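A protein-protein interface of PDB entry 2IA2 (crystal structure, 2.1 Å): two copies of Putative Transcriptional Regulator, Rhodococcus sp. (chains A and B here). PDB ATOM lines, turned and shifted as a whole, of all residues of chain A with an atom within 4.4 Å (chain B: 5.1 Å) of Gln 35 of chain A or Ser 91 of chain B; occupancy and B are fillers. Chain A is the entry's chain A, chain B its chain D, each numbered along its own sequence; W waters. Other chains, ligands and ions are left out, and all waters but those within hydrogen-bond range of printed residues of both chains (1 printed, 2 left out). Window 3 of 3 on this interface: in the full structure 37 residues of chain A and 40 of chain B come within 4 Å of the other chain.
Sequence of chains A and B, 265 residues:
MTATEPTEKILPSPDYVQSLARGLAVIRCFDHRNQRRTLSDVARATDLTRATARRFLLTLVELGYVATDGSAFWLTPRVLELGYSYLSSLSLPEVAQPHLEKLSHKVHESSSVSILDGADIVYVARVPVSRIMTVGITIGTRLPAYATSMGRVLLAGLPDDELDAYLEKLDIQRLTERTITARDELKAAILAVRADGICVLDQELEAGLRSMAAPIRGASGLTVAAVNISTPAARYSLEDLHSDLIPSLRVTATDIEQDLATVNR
A ring nitrogen (ND1) of His 32 of chain A sits at hydrogen-bond distance from the side-chain carboxylate of Glu 94 of chain B, at 3.4 Å.
The backbone NH of Arg 33 of chain A is in hydrogen-bond range of the side-chain carboxylate of Asp 31 of chain A (3.2 Å). OD1 of Asp 31 of chain A sits at hydrogen-bond distance from N of Asn 34 of chain A (2.9 Å). The side-chain hydroxyl (OG) of Ser 91 of chain B is in hydrogen-bond range of the side-chain amide oxygen (OD1) of Asn 264 of chain B (3.2 Å).
Asp 31 of chain A touches Ser 88 of chain B. Asp 31 of chain A touches Ser 89 of chain B. His 32 of chain A touches Ser 88 of chain B. Gln 35 of chain A touches Ser 89 of chain B. Ser 91 of chain B touches Gln 35 of chain A (OG to NE2, 3.96 Å).
Of chain B, only Ser 89 and Ser 91 come within 4 Å of Gln 35 of chain A. Of chain A, only Gln 35 comes within 4 Å of Ser 91 of chain B. Of the printed residues of chain B, His 32 of chain A touches Ser 88 and Glu 94. Of the printed residues of chain A, Ser 88 of chain B touches Asp 31 (3.4 Å) and His 32 (3.3 Å). Of the printed residues of chain B, Asp 31 of chain A touches Ser 88 (3.4 Å) and Ser 89 (3.4 Å). Printed residues of chain A within 4 Å of Glu 94 of chain B: His 32. Val 263 of chain B touches none of the printed residues of chain A. The nearest printed residue of chain A that does not touch Ser 89 of chain B is Phe 30 of chain A (4.1 Å).
Hydrophobic or aromatic side chains of chain A that line the printed part of chain B: His 32.
No position is printed for both chains.
Water W1 lies within hydrogen-bond range of the side-chain hydroxyl (OG) of Ser 89 of chain B and the backbone carbonyl oxygen (O) of Gln 35 of chain A.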
ATOM      1  N   PHE A  30      28.444  -0.160  15.113  1.00  0.00           N
ATOM      2  CA  PHE A  30      28.342   0.676  16.331  1.00  0.00           C
ATOM      3  C   PHE A  30      29.338   1.850  16.376  1.00  0.00           C
ATOM      4  O   PHE A  30      30.505   1.733  16.004  1.00  0.00           O
ATOM      5  CB  PHE A  30      28.432  -0.219  17.587  1.00  0.00           C
ATOM      6  CG  PHE A  30      27.437  -1.368  17.552  1.00  0.00           C
ATOM      7  CD1 PHE A  30      27.786  -2.563  16.980  1.00  0.00           C
ATOM      8  CD2 PHE A  30      26.127  -1.211  18.025  1.00  0.00           C
ATOM      9  CE1 PHE A  30      26.875  -3.639  16.858  1.00  0.00           C
ATOM     10  CE2 PHE A  30      25.172  -2.298  17.929  1.00  0.00           C
ATOM     11  CZ  PHE A  30      25.560  -3.502  17.377  1.00  0.00           C
ATOM     12  N   ASP A  31      28.872   3.004  16.785  1.00  0.00           N
ATOM     13  CA  ASP A  31      29.752   4.142  16.886  1.00  0.00           C
ATOM     14  C   ASP A  31      29.107   5.221  17.735  1.00  0.00           C
ATOM     15  O   ASP A  31      28.114   4.965  18.459  1.00  0.00           O
ATOM     16  CB  ASP A  31      30.104   4.666  15.503  1.00  0.00           C
ATOM     17  CG  ASP A  31      28.867   4.964  14.667  1.00  0.00           C
ATOM     18  OD1 ASP A  31      27.778   5.269  15.238  1.00  0.00           O
ATOM     19  OD2 ASP A  31      28.976   4.881  13.434  1.00  0.00           O
ATOM     20  N   HIS A  32      29.662   6.428  17.628  1.00  0.00           N
ATOM     21  CA  HIS A  32      29.216   7.506  18.490  1.00  0.00           C
ATOM     22  C   HIS A  32      27.726   7.845  18.267  1.00  0.00           C
ATOM     23  O   HIS A  32      26.969   8.098  19.214  1.00  0.00           O
ATOM     24  CB  HIS A  32      30.086   8.760  18.295  1.00  0.00           C
ATOM     25  CG  HIS A  32      29.529   9.961  18.975  1.00  0.00           C
ATOM     26  ND1 HIS A  32      29.684  10.191  20.326  1.00  0.00           N
ATOM     27  CD2 HIS A  32      28.781  10.991  18.501  1.00  0.00           C
ATOM     28  CE1 HIS A  32      29.073  11.318  20.652  1.00  0.00           C
ATOM     29  NE2 HIS A  32      28.530  11.832  19.561  1.00  0.00           N
ATOM     30  N   ARG A  33      27.320   7.843  17.008  1.00  0.00           N
ATOM     31  CA  ARG A  33      25.968   8.241  16.665  1.00  0.00           C
ATOM     32  C   ARG A  33      25.037   7.044  16.870  1.00  0.00           C
ATOM     33  O   ARG A  33      23.809   7.193  16.922  1.00  0.00           O
ATOM     34  CB  ARG A  33      25.906   8.791  15.203  1.00  0.00           C
ATOM     35  CG  ARG A  33      26.592  10.210  14.994  1.00  0.00           C
ATOM     36  N   ASN A  34      25.600   5.852  17.006  1.00  0.00           N
ATOM     37  CA  ASN A  34      24.771   4.624  17.012  1.00  0.00           C
ATOM     38  C   ASN A  34      25.227   3.663  18.094  1.00  0.00           C
ATOM     39  O   ASN A  34      25.865   2.633  17.797  1.00  0.00           O
ATOM     40  CB  ASN A  34      24.801   3.896  15.657  1.00  0.00           C
ATOM     41  CG  ASN A  34      24.252   4.733  14.529  1.00  0.00           C
ATOM     42  OD1 ASN A  34      23.059   4.662  14.215  1.00  0.00           O
ATOM     43  ND2 ASN A  34      25.122   5.521  13.886  1.00  0.00           N
ATOM     44  N   GLN A  35      24.874   3.986  19.341  1.00  0.00           N
ATOM     45  CA  GLN A  35      25.440   3.304  20.487  1.00  0.00           C
ATOM     46  C   GLN A  35      24.786   1.956  20.756  1.00  0.00           C
ATOM     47  O   GLN A  35      25.434   0.994  21.201  1.00  0.00           O
ATOM     48  CB  GLN A  35      25.262   4.187  21.715  1.00  0.00           C
ATOM     49  CG  GLN A  35      25.739   5.639  21.535  1.00  0.00           C
ATOM     50  CD  GLN A  35      25.770   6.372  22.880  1.00  0.00           C
ATOM     51  OE1 GLN A  35      24.973   6.078  23.784  1.00  0.00           O
ATOM     52  NE2 GLN A  35      26.715   7.304  23.029  1.00  0.00           N
ATOM     53  N   ARG A  36      23.476   1.925  20.552  1.00  0.00           N
ATOM     54  CA  ARG A  36      22.693   0.712  20.644  1.00  0.00           C
ATOM     55  C   ARG A  36      21.901   0.605  19.331  1.00  0.00           C
ATOM     56  O   ARG A  36      21.521   1.625  18.765  1.00  0.00           O
ATOM     57  CB  ARG A  36      21.735   0.758  21.843  1.00  0.00           C
ATOM     58  CG  ARG A  36      22.475   0.814  23.186  1.00  0.00           C
ATOM     59  CD  ARG A  36      21.575   0.461  24.399  1.00  0.00           C
ATOM     60  NE  ARG A  36      22.427   0.134  25.570  1.00  0.00           N
ATOM     61  CZ  ARG A  36      22.006  -0.456  26.697  1.00  0.00           C
ATOM     62  NH1 ARG A  36      20.724  -0.803  26.845  1.00  0.00           N
ATOM     63  NH2 ARG A  36      22.869  -0.704  27.683  1.00  0.00           N
ATOM     64  N   TRP A  74      24.329  -4.103  21.711  1.00  0.00           N
ATOM     65  CA  TRP A  74      25.446  -3.183  21.821  1.00  0.00           C
ATOM     66  C   TRP A  74      26.734  -3.971  22.062  1.00  0.00           C
ATOM     67  O   TRP A  74      26.692  -5.160  22.329  1.00  0.00           O
ATOM     68  CB  TRP A  74      25.214  -2.170  22.967  1.00  0.00           C
ATOM     69  CG  TRP A  74      24.994  -2.839  24.284  1.00  0.00           C
ATOM     70  CD1 TRP A  74      25.954  -3.139  25.227  1.00  0.00           C
ATOM     71  CD2 TRP A  74      23.745  -3.333  24.820  1.00  0.00           C
ATOM     72  NE1 TRP A  74      25.383  -3.766  26.303  1.00  0.00           N
ATOM     73  CE2 TRP A  74      24.037  -3.901  26.092  1.00  0.00           C
ATOM     74  CE3 TRP A  74      22.412  -3.357  24.348  1.00  0.00           C
ATOM     75  CZ2 TRP A  74      23.037  -4.482  26.919  1.00  0.00           C
ATOM     76  CZ3 TRP A  74      21.424  -3.927  25.163  1.00  0.00           C
ATOM     77  CH2 TRP A  74      21.743  -4.480  26.440  1.00  0.00           C
ATOM     78  N   SER B  88      33.857   4.139  21.067  1.00  0.00           N
ATOM     79  CA  SER B  88      33.157   5.315  20.564  1.00  0.00           C
ATOM     80  C   SER B  88      31.664   5.237  20.861  1.00  0.00           C
ATOM     81  O   SER B  88      30.992   6.261  20.986  1.00  0.00           O
ATOM     82  CB  SER B  88      33.386   5.473  19.059  1.00  0.00           C
ATOM     83  OG  SER B  88      32.809   4.397  18.340  1.00  0.00           O
ATOM     84  N   SER B  89      31.151   4.016  20.973  1.00  0.00           N
ATOM     85  CA  SER B  89      29.728   3.801  21.175  1.00  0.00           C
ATOM     86  C   SER B  89      29.397   3.857  22.656  1.00  0.00           C
ATOM     87  O   SER B  89      28.269   4.042  22.996  1.00  0.00           O
ATOM     88  CB  SER B  89      29.241   2.491  20.517  1.00  0.00           C
ATOM     89  OG  SER B  89      29.656   1.382  21.250  1.00  0.00           O
ATOM     90  N   LEU B  90      30.375   3.700  23.518  1.00  0.00           N
ATOM     91  CA  LEU B  90      30.327   4.129  24.912  1.00  0.00           C
ATOM     92  C   LEU B  90      30.401   5.675  25.048  1.00  0.00           C
ATOM     93  O   LEU B  90      31.156   6.277  24.385  1.00  0.00           O
ATOM     94  CB  LEU B  90      31.510   3.466  25.599  1.00  0.00           C
ATOM     95  CG  LEU B  90      31.499   2.829  26.973  1.00  0.00           C
ATOM     96  CD1 LEU B  90      30.448   1.782  27.153  1.00  0.00           C
ATOM     97  CD2 LEU B  90      32.876   2.333  27.403  1.00  0.00           C
ATOM     98  N   SER B  91      29.614   6.312  25.904  1.00  0.00           N
ATOM     99  CA  SER B  91      29.744   7.789  26.079  1.00  0.00           C
ATOM    100  C   SER B  91      31.122   8.092  26.734  1.00  0.00           C
ATOM    101  O   SER B  91      31.867   8.947  26.290  1.00  0.00           O
ATOM    102  CB  SER B  91      28.702   8.364  27.038  1.00  0.00           C
ATOM    103  OG  SER B  91      27.424   7.775  26.895  1.00  0.00           O
ATOM    104  N   LEU B  92      31.459   7.336  27.776  1.00  0.00           N
ATOM    105  CA  LEU B  92      32.575   7.703  28.638  1.00  0.00           C
ATOM    106  C   LEU B  92      33.958   8.007  27.937  1.00  0.00           C
ATOM    107  O   LEU B  92      34.555   9.036  28.192  1.00  0.00           O
ATOM    108  CB  LEU B  92      32.668   6.685  29.813  1.00  0.00           C
ATOM    109  CG  LEU B  92      33.877   6.893  30.715  1.00  0.00           C
ATOM    110  CD1 LEU B  92      33.710   8.163  31.530  1.00  0.00           C
ATOM    111  CD2 LEU B  92      34.155   5.664  31.611  1.00  0.00           C
ATOM    112  N   PRO B  93      34.515   7.082  27.110  1.00  0.00           N
ATOM    113  CA  PRO B  93      35.902   7.299  26.672  1.00  0.00           C
ATOM    114  C   PRO B  93      36.158   8.638  26.001  1.00  0.00           C
ATOM    115  O   PRO B  93      37.094   9.318  26.358  1.00  0.00           O
ATOM    116  CB  PRO B  93      36.139   6.105  25.683  1.00  0.00           C
ATOM    117  CG  PRO B  93      35.282   5.003  26.314  1.00  0.00           C
ATOM    118  CD  PRO B  93      33.987   5.819  26.559  1.00  0.00           C
ATOM    119  N   GLU B  94      35.326   9.019  25.026  1.00  0.00           N
ATOM    120  CA  GLU B  94      35.493  10.304  24.312  1.00  0.00           C
ATOM    121  C   GLU B  94      35.075  11.504  25.121  1.00  0.00           C
ATOM    122  O   GLU B  94      35.589  12.603  24.878  1.00  0.00           O
ATOM    123  CB  GLU B  94      34.612  10.278  23.072  1.00  0.00           C
ATOM    124  CG  GLU B  94      35.123   9.253  22.042  1.00  0.00           C
ATOM    125  CD  GLU B  94      34.228   9.227  20.746  1.00  0.00           C
ATOM    126  OE1 GLU B  94      32.930   9.291  20.813  1.00  0.00           O
ATOM    127  OE2 GLU B  94      34.864   9.124  19.681  1.00  0.00           O
ATOM    128  N   VAL B  95      34.152  11.310  26.087  1.00  0.00           N
ATOM    129  CA  VAL B  95      33.800  12.401  27.034  1.00  0.00           C
ATOM    130  C   VAL B  95      35.005  12.736  27.928  1.00  0.00           C
ATOM    131  O   VAL B  95      35.284  13.876  28.184  1.00  0.00           O
ATOM    132  CB  VAL B  95      32.557  12.051  27.927  1.00  0.00           C
ATOM    133  CG1 VAL B  95      32.549  12.928  29.200  1.00  0.00           C
ATOM    134  CG2 VAL B  95      31.232  12.326  27.116  1.00  0.00           C
ATOM    135  N   LEU B 260      29.470  13.813  31.453  1.00  0.00           N
ATOM    136  CA  LEU B 260      28.782  12.564  31.287  1.00  0.00           C
ATOM    137  C   LEU B 260      27.274  12.720  31.505  1.00  0.00           C
ATOM    138  O   LEU B 260      26.486  12.147  30.752  1.00  0.00           O
ATOM    139  CB  LEU B 260      29.367  11.542  32.290  1.00  0.00           C
ATOM    140  CG  LEU B 260      29.350  10.049  31.995  1.00  0.00           C
ATOM    141  CD1 LEU B 260      29.984   9.709  30.634  1.00  0.00           C
ATOM    142  CD2 LEU B 260      30.042   9.244  33.171  1.00  0.00           C
ATOM    143  N   VAL B 263      25.490  14.304  28.436  1.00  0.00           N
ATOM    144  CA  VAL B 263      25.377  13.437  27.255  1.00  0.00           C
ATOM    145  C   VAL B 263      24.357  12.320  27.444  1.00  0.00           C
ATOM    146  O   VAL B 263      23.881  11.745  26.449  1.00  0.00           O
ATOM    147  CB  VAL B 263      26.766  12.863  26.702  1.00  0.00           C
ATOM    148  CG1 VAL B 263      27.785  13.991  26.369  1.00  0.00           C
ATOM    149  CG2 VAL B 263      27.372  11.834  27.609  1.00  0.00           C
ATOM    150  N   ASN B 264      23.978  12.041  28.692  1.00  0.00           N
ATOM    151  CA  ASN B 264      23.012  10.958  28.976  1.00  0.00           C
ATOM    152  C   ASN B 264      21.588  11.420  29.372  1.00  0.00           C
ATOM    153  O   ASN B 264      21.315  12.620  29.463  1.00  0.00           O
ATOM    154  CB  ASN B 264      23.582   9.973  30.014  1.00  0.00           C
ATOM    155  CG  ASN B 264      24.725   9.107  29.451  1.00  0.00           C
ATOM    156  OD1 ASN B 264      24.672   8.627  28.306  1.00  0.00           O
ATOM    157  ND2 ASN B 264      25.765   8.919  30.254  1.00  0.00           N
HETATM  158  O   HOH W   1      27.711  -0.494  21.450  1.00  0.00           O
